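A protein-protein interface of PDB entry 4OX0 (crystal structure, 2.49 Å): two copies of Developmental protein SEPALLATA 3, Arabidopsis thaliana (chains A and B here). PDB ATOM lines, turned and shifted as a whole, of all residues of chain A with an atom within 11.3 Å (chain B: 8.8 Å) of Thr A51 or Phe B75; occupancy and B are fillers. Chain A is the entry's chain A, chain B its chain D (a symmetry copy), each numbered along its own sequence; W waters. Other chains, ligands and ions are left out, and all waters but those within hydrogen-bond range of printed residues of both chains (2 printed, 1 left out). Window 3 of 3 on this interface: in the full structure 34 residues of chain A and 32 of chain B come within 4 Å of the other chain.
The side-chain carboxylate (OE2) of Glu A55 is in salt-bridge range of the guanidinium group (NH1) of Arg B72. NE of Arg B72 lies within salt-bridge range of OE1 of Glu A58, at 2.9 Å.
The side-chain amino group of Lys A52 is in salt-bridge range of the side-chain carboxylate of Glu A55, 2.9 Å away. O of Arg B69 is in hydrogen-bond range of OG1 of Thr B73.
Among the printed residues, merely in contact across the chains: Glu A58 with Arg B69 (3.4 Å), Leu A46 with Leu B71 (3.5 Å), Leu A54 with Ile B68 (3.6 Å), Thr A51 with Phe B75 (3.7 Å), Leu A46 with Ile B68 (3.7 Å), Leu A54 with Leu B71 (3.7 Å), Glu A58 with Ile B68 (3.9 Å) and Leu A57 with Ile B68 (3.9 Å).
No residue of chain B comes within 4 Å of Ser A50. Thr A51 touches just one residue of chain B: Phe B75. Printed residues of chain B within 4 Å of Leu A54: Ile B68 (3.6 Å) and Leu B71 (3.7 Å). Printed residues of chain B within 4 Å of Glu A55: Arg B72. Printed residues of chain A within 4 Å of Ile B68: Leu A46 (3.7 Å), Leu A54 (3.6 Å), Leu A57 (3.9 Å) and Glu A58 (3.9 Å). Of the printed residues of chain A, Arg B69 touches Glu A58 (3.4 Å). Leu B71 touches just these residues of chain A: Leu A46 (3.5 Å) and Leu A54 (3.7 Å). Printed residues of chain A within 4 Å of Arg B72: Glu A55 and Glu A58. No residue of chain A comes within 4 Å of Gln B74. Phe B75 touches one residue of chain A. No residue of chain A comes within 4 Å of Met B76. No residue of chain A comes within 4 Å of Asp B78. Gln B79 touches none of the printed residues of chain A. The nearest residue of chain B that does not touch Thr A51 is Arg B72 (5.0 Å).
Of the 15 printed residues of chain B, 5 touch a printed residue of chain A. Hydrophobic or aromatic side chains of chain B that line the printed part of chain A: Ile B68, Leu B71 and Phe B75. Among the printed residues, Asp or Glu carboxylates within 4 Å of a Lys or Arg side-chain nitrogen of the other chain: Glu A55 with Arg B72 and Glu A58 with Arg B72.
No position is printed for both chains. Of the 10 pairs that touch across the chains among the printed residues, none has its exchanged pair printed and touching as well.
Water W1 bridges the guanidinium group (NH2) of Arg B72 (2.9 Å) and the side-chain carboxylate (OE2) of Glu A58 (3.4 Å). Water W2 lies within hydrogen-bond range of the side-chain carboxylate of Glu A55 and the guanidinium group of Arg B72.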
ATOM      1  N   LEU A  46     -19.111  19.611 -12.232  1.00  0.00           N
ATOM      2  CA  LEU A  46     -20.475  19.273 -12.635  1.00  0.00           C
ATOM      3  C   LEU A  46     -20.635  18.611 -13.994  1.00  0.00           C
ATOM      4  O   LEU A  46     -21.694  18.041 -14.246  1.00  0.00           O
ATOM      5  CB  LEU A  46     -21.393  20.481 -12.477  1.00  0.00           C
ATOM      6  CG  LEU A  46     -21.522  21.083 -11.069  1.00  0.00           C
ATOM      7  CD1 LEU A  46     -22.228  22.392 -11.140  1.00  0.00           C
ATOM      8  CD2 LEU A  46     -22.252  20.153 -10.113  1.00  0.00           C
ATOM      9  N   GLY A  47     -19.576  18.651 -14.816  1.00  0.00           N
ATOM     10  CA  GLY A  47     -19.503  18.096 -16.168  1.00  0.00           C
ATOM     11  C   GLY A  47     -19.941  16.651 -16.360  1.00  0.00           C
ATOM     12  O   GLY A  47     -20.763  16.393 -17.243  1.00  0.00           O
ATOM     13  N   PRO A  48     -19.429  15.670 -15.573  1.00  0.00           N
ATOM     14  CA  PRO A  48     -19.855  14.268 -15.758  1.00  0.00           C
ATOM     15  C   PRO A  48     -21.339  13.968 -15.523  1.00  0.00           C
ATOM     16  O   PRO A  48     -21.840  12.951 -16.002  1.00  0.00           O
ATOM     17  CB  PRO A  48     -19.005  13.507 -14.735  1.00  0.00           C
ATOM     18  CG  PRO A  48     -17.880  14.402 -14.418  1.00  0.00           C
ATOM     19  CD  PRO A  48     -18.431  15.772 -14.494  1.00  0.00           C
ATOM     20  N   LEU A  49     -22.034  14.843 -14.778  1.00  0.00           N
ATOM     21  CA  LEU A  49     -23.441  14.697 -14.403  1.00  0.00           C
ATOM     22  C   LEU A  49     -24.446  14.863 -15.549  1.00  0.00           C
ATOM     23  O   LEU A  49     -24.353  15.806 -16.329  1.00  0.00           O
ATOM     24  CB  LEU A  49     -23.794  15.684 -13.284  1.00  0.00           C
ATOM     25  CG  LEU A  49     -23.235  15.504 -11.875  1.00  0.00           C
ATOM     26  CD1 LEU A  49     -23.821  16.553 -11.011  1.00  0.00           C
ATOM     27  CD2 LEU A  49     -23.581  14.152 -11.242  1.00  0.00           C
ATOM     28  N   SER A  50     -25.420  13.951 -15.622  1.00  0.00           N
ATOM     29  CA  SER A  50     -26.473  14.009 -16.627  1.00  0.00           C
ATOM     30  C   SER A  50     -27.426  15.107 -16.236  1.00  0.00           C
ATOM     31  O   SER A  50     -27.503  15.437 -15.048  1.00  0.00           O
ATOM     32  CB  SER A  50     -27.217  12.682 -16.705  1.00  0.00           C
ATOM     33  OG  SER A  50     -27.763  12.301 -15.454  1.00  0.00           O
ATOM     34  N   THR A  51     -28.157  15.682 -17.211  1.00  0.00           N
ATOM     35  CA  THR A  51     -29.101  16.776 -16.940  1.00  0.00           C
ATOM     36  C   THR A  51     -30.158  16.416 -15.910  1.00  0.00           C
ATOM     37  O   THR A  51     -30.647  17.302 -15.235  1.00  0.00           O
ATOM     38  CB  THR A  51     -29.624  17.451 -18.220  1.00  0.00           C
ATOM     39  OG1 THR A  51     -30.951  17.013 -18.511  1.00  0.00           O
ATOM     40  CG2 THR A  51     -28.692  17.264 -19.418  1.00  0.00           C
ATOM     41  N   LYS A  52     -30.445  15.121 -15.734  1.00  0.00           N
ATOM     42  CA  LYS A  52     -31.388  14.607 -14.745  1.00  0.00           C
ATOM     43  C   LYS A  52     -30.756  14.605 -13.359  1.00  0.00           C
ATOM     44  O   LYS A  52     -31.420  15.014 -12.394  1.00  0.00           O
ATOM     45  CB  LYS A  52     -31.912  13.212 -15.138  1.00  0.00           C
ATOM     46  CG  LYS A  52     -32.880  13.222 -16.349  1.00  0.00           C
ATOM     47  CD  LYS A  52     -34.212  13.987 -16.088  1.00  0.00           C
ATOM     48  CE  LYS A  52     -34.805  14.600 -17.342  1.00  0.00           C
ATOM     49  NZ  LYS A  52     -35.661  15.782 -17.036  1.00  0.00           N
ATOM     50  N   GLU A  53     -29.473  14.177 -13.264  1.00  0.00           N
ATOM     51  CA  GLU A  53     -28.694  14.194 -12.032  1.00  0.00           C
ATOM     52  C   GLU A  53     -28.497  15.652 -11.581  1.00  0.00           C
ATOM     53  O   GLU A  53     -28.569  15.936 -10.381  1.00  0.00           O
ATOM     54  CB  GLU A  53     -27.307  13.580 -12.253  1.00  0.00           C
ATOM     55  CG  GLU A  53     -27.252  12.065 -12.243  1.00  0.00           C
ATOM     56  CD  GLU A  53     -25.884  11.488 -12.555  1.00  0.00           C
ATOM     57  OE1 GLU A  53     -25.259  11.938 -13.541  1.00  0.00           O
ATOM     58  OE2 GLU A  53     -25.455  10.556 -11.839  1.00  0.00           O
ATOM     59  N   LEU A  54     -28.218  16.553 -12.545  1.00  0.00           N
ATOM     60  CA  LEU A  54     -27.981  17.978 -12.337  1.00  0.00           C
ATOM     61  C   LEU A  54     -29.228  18.687 -11.833  1.00  0.00           C
ATOM     62  O   LEU A  54     -29.121  19.615 -11.036  1.00  0.00           O
ATOM     63  CB  LEU A  54     -27.496  18.576 -13.662  1.00  0.00           C
ATOM     64  CG  LEU A  54     -26.653  19.849 -13.640  1.00  0.00           C
ATOM     65  CD1 LEU A  54     -25.381  19.693 -12.785  1.00  0.00           C
ATOM     66  CD2 LEU A  54     -26.273  20.237 -15.053  1.00  0.00           C
ATOM     67  N   GLU A  55     -30.409  18.236 -12.269  1.00  0.00           N
ATOM     68  CA  GLU A  55     -31.715  18.744 -11.849  1.00  0.00           C
ATOM     69  C   GLU A  55     -32.038  18.276 -10.433  1.00  0.00           C
ATOM     70  O   GLU A  55     -32.546  19.062  -9.646  1.00  0.00           O
ATOM     71  CB  GLU A  55     -32.799  18.253 -12.828  1.00  0.00           C
ATOM     72  CG  GLU A  55     -32.998  19.152 -14.028  1.00  0.00           C
ATOM     73  CD  GLU A  55     -33.625  18.530 -15.265  1.00  0.00           C
ATOM     74  OE1 GLU A  55     -34.582  17.730 -15.138  1.00  0.00           O
ATOM     75  OE2 GLU A  55     -33.203  18.921 -16.379  1.00  0.00           O
ATOM     76  N   SER A  56     -31.744  16.996 -10.113  1.00  0.00           N
ATOM     77  CA  SER A  56     -31.962  16.376  -8.796  1.00  0.00           C
ATOM     78  C   SER A  56     -31.121  17.075  -7.715  1.00  0.00           C
ATOM     79  O   SER A  56     -31.623  17.320  -6.616  1.00  0.00           O
ATOM     80  CB  SER A  56     -31.661  14.876  -8.859  1.00  0.00           C
ATOM     81  OG  SER A  56     -31.494  14.252  -7.588  1.00  0.00           O
ATOM     82  N   LEU A  57     -29.864  17.415  -8.045  1.00  0.00           N
ATOM     83  CA  LEU A  57     -28.924  18.116  -7.184  1.00  0.00           C
ATOM     84  C   LEU A  57     -29.464  19.518  -6.866  1.00  0.00           C
ATOM     85  O   LEU A  57     -29.430  19.937  -5.721  1.00  0.00           O
ATOM     86  CB  LEU A  57     -27.573  18.206  -7.911  1.00  0.00           C
ATOM     87  CG  LEU A  57     -26.447  18.948  -7.246  1.00  0.00           C
ATOM     88  CD1 LEU A  57     -26.069  18.345  -5.925  1.00  0.00           C
ATOM     89  CD2 LEU A  57     -25.256  18.915  -8.128  1.00  0.00           C
ATOM     90  N   GLU A  58     -29.989  20.213  -7.879  1.00  0.00           N
ATOM     91  CA  GLU A  58     -30.565  21.535  -7.754  1.00  0.00           C
ATOM     92  C   GLU A  58     -31.744  21.531  -6.793  1.00  0.00           C
ATOM     93  O   GLU A  58     -31.848  22.425  -5.960  1.00  0.00           O
ATOM     94  CB  GLU A  58     -31.028  22.009  -9.137  1.00  0.00           C
ATOM     95  CG  GLU A  58     -31.331  23.489  -9.167  1.00  0.00           C
ATOM     96  CD  GLU A  58     -32.058  24.014 -10.389  1.00  0.00           C
ATOM     97  OE1 GLU A  58     -32.006  23.343 -11.443  1.00  0.00           O
ATOM     98  OE2 GLU A  58     -32.698  25.090 -10.287  1.00  0.00           O
ATOM     99  N   ARG A  59     -32.625  20.537  -6.913  1.00  0.00           N
ATOM    100  CA  ARG A  59     -33.792  20.401  -6.046  1.00  0.00           C
ATOM    101  C   ARG A  59     -33.394  20.110  -4.601  1.00  0.00           C
ATOM    102  O   ARG A  59     -34.055  20.586  -3.693  1.00  0.00           O
ATOM    103  CB  ARG A  59     -34.702  19.282  -6.539  1.00  0.00           C
ATOM    104  CG  ARG A  59     -35.524  19.626  -7.754  1.00  0.00           C
ATOM    105  CD  ARG A  59     -36.570  18.565  -7.982  1.00  0.00           C
ATOM    106  NE  ARG A  59     -35.997  17.227  -8.125  1.00  0.00           N
ATOM    107  CZ  ARG A  59     -35.746  16.643  -9.290  1.00  0.00           C
ATOM    108  NH1 ARG A  59     -36.033  17.266 -10.424  1.00  0.00           N
ATOM    109  NH2 ARG A  59     -35.226  15.423  -9.329  1.00  0.00           N
ATOM    110  N   GLN A  60     -32.339  19.311  -4.402  1.00  0.00           N
ATOM    111  CA  GLN A  60     -31.779  18.919  -3.110  1.00  0.00           C
ATOM    112  C   GLN A  60     -31.186  20.153  -2.422  1.00  0.00           C
ATOM    113  O   GLN A  60     -31.500  20.423  -1.255  1.00  0.00           O
ATOM    114  CB  GLN A  60     -30.675  17.855  -3.325  1.00  0.00           C
ATOM    115  CG  GLN A  60     -30.739  16.635  -2.409  1.00  0.00           C
ATOM    116  CD  GLN A  60     -29.880  15.462  -2.905  1.00  0.00           C
ATOM    117  OE1 GLN A  60     -28.889  15.611  -3.645  1.00  0.00           O
ATOM    118  NE2 GLN A  60     -30.221  14.252  -2.475  1.00  0.00           N
ATOM    119  N   ILE B  68     -24.948  25.697 -10.867  1.00  0.00           N
ATOM    120  CA  ILE B  68     -25.756  24.631 -11.445  1.00  0.00           C
ATOM    121  C   ILE B  68     -26.691  25.251 -12.472  1.00  0.00           C
ATOM    122  O   ILE B  68     -26.750  24.800 -13.615  1.00  0.00           O
ATOM    123  CB  ILE B  68     -26.503  23.840 -10.327  1.00  0.00           C
ATOM    124  CG1 ILE B  68     -25.497  23.021  -9.497  1.00  0.00           C
ATOM    125  CG2 ILE B  68     -27.684  22.960 -10.867  1.00  0.00           C
ATOM    126  CD1 ILE B  68     -25.934  22.775  -8.118  1.00  0.00           C
ATOM    127  N   ARG B  69     -27.388  26.302 -12.072  1.00  0.00           N
ATOM    128  CA  ARG B  69     -28.301  26.999 -12.966  1.00  0.00           C
ATOM    129  C   ARG B  69     -27.591  27.632 -14.177  1.00  0.00           C
ATOM    130  O   ARG B  69     -28.117  27.515 -15.272  1.00  0.00           O
ATOM    131  CB  ARG B  69     -29.211  27.961 -12.207  1.00  0.00           C
ATOM    132  CG  ARG B  69     -30.207  27.210 -11.307  1.00  0.00           C
ATOM    133  CD  ARG B  69     -31.225  28.089 -10.577  1.00  0.00           C
ATOM    134  NE  ARG B  69     -30.610  29.281  -9.993  1.00  0.00           N
ATOM    135  CZ  ARG B  69     -30.571  29.557  -8.691  1.00  0.00           C
ATOM    136  NH1 ARG B  69     -31.185  28.768  -7.821  1.00  0.00           N
ATOM    137  NH2 ARG B  69     -29.948  30.645  -8.256  1.00  0.00           N
ATOM    138  N   ALA B  70     -26.369  28.190 -14.011  1.00  0.00           N
ATOM    139  CA  ALA B  70     -25.565  28.752 -15.101  1.00  0.00           C
ATOM    140  C   ALA B  70     -25.154  27.652 -16.061  1.00  0.00           C
ATOM    141  O   ALA B  70     -25.098  27.907 -17.254  1.00  0.00           O
ATOM    142  CB  ALA B  70     -24.327  29.450 -14.567  1.00  0.00           C
ATOM    143  N   LEU B  71     -24.920  26.420 -15.558  1.00  0.00           N
ATOM    144  CA  LEU B  71     -24.576  25.259 -16.369  1.00  0.00           C
ATOM    145  C   LEU B  71     -25.775  24.761 -17.157  1.00  0.00           C
ATOM    146  O   LEU B  71     -25.652  24.556 -18.361  1.00  0.00           O
ATOM    147  CB  LEU B  71     -23.987  24.147 -15.498  1.00  0.00           C
ATOM    148  CG  LEU B  71     -23.379  22.946 -16.229  1.00  0.00           C
ATOM    149  CD1 LEU B  71     -22.237  23.360 -17.171  1.00  0.00           C
ATOM    150  CD2 LEU B  71     -22.931  21.922 -15.256  1.00  0.00           C
ATOM    151  N   ARG B  72     -26.930  24.589 -16.512  1.00  0.00           N
ATOM    152  CA  ARG B  72     -28.169  24.178 -17.189  1.00  0.00           C
ATOM    153  C   ARG B  72     -28.513  25.174 -18.339  1.00  0.00           C
ATOM    154  O   ARG B  72     -28.864  24.742 -19.436  1.00  0.00           O
ATOM    155  CB  ARG B  72     -29.355  24.100 -16.183  1.00  0.00           C
ATOM    156  CG  ARG B  72     -29.205  23.105 -15.022  1.00  0.00           C
ATOM    157  CD  ARG B  72     -30.463  22.307 -14.815  1.00  0.00           C
ATOM    158  NE  ARG B  72     -31.563  23.136 -14.340  1.00  0.00           N
ATOM    159  CZ  ARG B  72     -32.837  23.013 -14.710  1.00  0.00           C
ATOM    160  NH1 ARG B  72     -33.188  22.121 -15.625  1.00  0.00           N
ATOM    161  NH2 ARG B  72     -33.765  23.796 -14.182  1.00  0.00           N
ATOM    162  N   THR B  73     -28.375  26.497 -18.082  1.00  0.00           N
ATOM    163  CA  THR B  73     -28.632  27.564 -19.052  1.00  0.00           C
ATOM    164  C   THR B  73     -27.643  27.484 -20.224  1.00  0.00           C
ATOM    165  O   THR B  73     -28.077  27.555 -21.373  1.00  0.00           O
ATOM    166  CB  THR B  73     -28.663  28.929 -18.362  1.00  0.00           C
ATOM    167  OG1 THR B  73     -29.825  28.977 -17.532  1.00  0.00           O
ATOM    168  CG2 THR B  73     -28.699  30.112 -19.346  1.00  0.00           C
ATOM    169  N   GLN B  74     -26.335  27.321 -19.944  1.00  0.00           N
ATOM    170  CA  GLN B  74     -25.302  27.244 -20.972  1.00  0.00           C
ATOM    171  C   GLN B  74     -25.464  26.019 -21.834  1.00  0.00           C
ATOM    172  O   GLN B  74     -25.295  26.117 -23.047  1.00  0.00           O
ATOM    173  CB  GLN B  74     -23.894  27.320 -20.379  1.00  0.00           C
ATOM    174  CG  GLN B  74     -22.822  27.818 -21.369  1.00  0.00           C
ATOM    175  CD  GLN B  74     -23.239  28.981 -22.267  1.00  0.00           C
ATOM    176  OE1 GLN B  74     -23.369  28.831 -23.489  1.00  0.00           O
ATOM    177  NE2 GLN B  74     -23.475  30.155 -21.694  1.00  0.00           N
ATOM    178  N   PHE B  75     -25.843  24.884 -21.222  1.00  0.00           N
ATOM    179  CA  PHE B  75     -26.113  23.630 -21.922  1.00  0.00           C
ATOM    180  C   PHE B  75     -27.281  23.835 -22.919  1.00  0.00           C
ATOM    181  O   PHE B  75     -27.173  23.414 -24.064  1.00  0.00           O
ATOM    182  CB  PHE B  75     -26.430  22.514 -20.910  1.00  0.00           C
ATOM    183  CG  PHE B  75     -26.703  21.165 -21.528  1.00  0.00           C
ATOM    184  CD1 PHE B  75     -25.654  20.346 -21.944  1.00  0.00           C
ATOM    185  CD2 PHE B  75     -28.010  20.711 -21.712  1.00  0.00           C
ATOM    186  CE1 PHE B  75     -25.905  19.110 -22.559  1.00  0.00           C
ATOM    187  CE2 PHE B  75     -28.261  19.472 -22.324  1.00  0.00           C
ATOM    188  CZ  PHE B  75     -27.207  18.677 -22.734  1.00  0.00           C
ATOM    189  N   MET B  76     -28.371  24.527 -22.487  1.00  0.00           N
ATOM    190  CA  MET B  76     -29.533  24.796 -23.337  1.00  0.00           C
ATOM    191  C   MET B  76     -29.190  25.714 -24.487  1.00  0.00           C
ATOM    192  O   MET B  76     -29.584  25.438 -25.605  1.00  0.00           O
ATOM    193  CB  MET B  76     -30.718  25.344 -22.534  1.00  0.00           C
ATOM    194  CG  MET B  76     -31.417  24.300 -21.717  1.00  0.00           C
ATOM    195  SD  MET B  76     -31.945  22.931 -22.747  1.00  0.00           S
ATOM    196  CE  MET B  76     -31.516  21.573 -21.664  1.00  0.00           C
ATOM    197  N   LEU B  77     -28.410  26.772 -24.216  1.00  0.00           N
ATOM    198  CA  LEU B  77     -27.948  27.742 -25.196  1.00  0.00           C
ATOM    199  C   LEU B  77     -27.050  27.112 -26.225  1.00  0.00           C
ATOM    200  O   LEU B  77     -27.162  27.463 -27.386  1.00  0.00           O
ATOM    201  CB  LEU B  77     -27.208  28.899 -24.518  1.00  0.00           C
ATOM    202  CG  LEU B  77     -28.067  29.972 -23.869  1.00  0.00           C
ATOM    203  CD1 LEU B  77     -27.227  30.844 -23.021  1.00  0.00           C
ATOM    204  CD2 LEU B  77     -28.800  30.827 -24.907  1.00  0.00           C
ATOM    205  N   ASP B  78     -26.185  26.176 -25.827  1.00  0.00           N
ATOM    206  CA  ASP B  78     -25.274  25.476 -26.734  1.00  0.00           C
ATOM    207  C   ASP B  78     -26.065  24.580 -27.701  1.00  0.00           C
ATOM    208  O   ASP B  78     -25.772  24.562 -28.901  1.00  0.00           O
ATOM    209  CB  ASP B  78     -24.230  24.662 -25.940  1.00  0.00           C
ATOM    210  CG  ASP B  78     -23.125  25.467 -25.261  1.00  0.00           C
ATOM    211  OD1 ASP B  78     -22.929  26.652 -25.632  1.00  0.00           O
ATOM    212  OD2 ASP B  78     -22.425  24.896 -24.386  1.00  0.00           O
ATOM    213  N   GLN B  79     -27.091  23.881 -27.178  1.00  0.00           N
ATOM    214  CA  GLN B  79     -27.984  23.013 -27.944  1.00  0.00           C
ATOM    215  C   GLN B  79     -28.798  23.823 -28.959  1.00  0.00           C
ATOM    216  O   GLN B  79     -28.969  23.401 -30.104  1.00  0.00           O
ATOM    217  CB  GLN B  79     -28.945  22.286 -26.997  1.00  0.00           C
ATOM    218  CG  GLN B  79     -28.353  21.142 -26.198  1.00  0.00           C
ATOM    219  CD  GLN B  79     -29.489  20.359 -25.586  1.00  0.00           C
ATOM    220  OE1 GLN B  79     -30.096  20.761 -24.580  1.00  0.00           O
ATOM    221  NE2 GLN B  79     -29.856  19.254 -26.224  1.00  0.00           N
ATOM    222  N   LEU B  80     -29.296  24.984 -28.525  1.00  0.00           N
ATOM    223  CA  LEU B  80     -30.075  25.904 -29.340  1.00  0.00           C
ATOM    224  C   LEU B  80     -29.221  26.485 -30.454  1.00  0.00           C
ATOM    225  O   LEU B  80     -29.696  26.504 -31.589  1.00  0.00           O
ATOM    226  CB  LEU B  80     -30.748  27.016 -28.500  1.00  0.00           C
ATOM    227  CG  LEU B  80     -31.939  26.567 -27.592  1.00  0.00           C
ATOM    228  CD1 LEU B  80     -32.358  27.662 -26.579  1.00  0.00           C
ATOM    229  CD2 LEU B  80     -33.129  26.070 -28.403  1.00  0.00           C
ATOM    230  N   ASN B  81     -27.951  26.898 -30.162  1.00  0.00           N
ATOM    231  CA  ASN B  81     -27.044  27.434 -31.186  1.00  0.00           C
ATOM    232  C   ASN B  81     -26.713  26.385 -32.241  1.00  0.00           C
ATOM    233  O   ASN B  81     -26.679  26.709 -33.429  1.00  0.00           O
ATOM    234  CB  ASN B  81     -25.770  28.033 -30.607  1.00  0.00           C
ATOM    235  CG  ASN B  81     -25.948  29.387 -29.952  1.00  0.00           C
ATOM    236  OD1 ASN B  81     -25.552  29.594 -28.796  1.00  0.00           O
ATOM    237  ND2 ASN B  81     -26.490  30.361 -30.679  1.00  0.00           N
ATOM    238  N   ASP B  82     -26.536  25.124 -31.811  1.00  0.00           N
ATOM    239  CA  ASP B  82     -26.242  23.993 -32.680  1.00  0.00           C
ATOM    240  C   ASP B  82     -27.405  23.728 -33.654  1.00  0.00           C
ATOM    241  O   ASP B  82     -27.174  23.561 -34.864  1.00  0.00           O
ATOM    242  CB  ASP B  82     -25.917  22.752 -31.831  1.00  0.00           C
ATOM    243  CG  ASP B  82     -25.470  21.563 -32.644  1.00  0.00           C
ATOM    244  OD1 ASP B  82     -24.344  21.605 -33.186  1.00  0.00           O
ATOM    245  OD2 ASP B  82     -26.242  20.584 -32.733  1.00  0.00           O
HETATM  246  O   HOH W   1     -34.736  26.127 -12.744  1.00  0.00           O
HETATM  247  O   HOH W   2     -31.587  20.874 -18.069  1.00  0.00           O
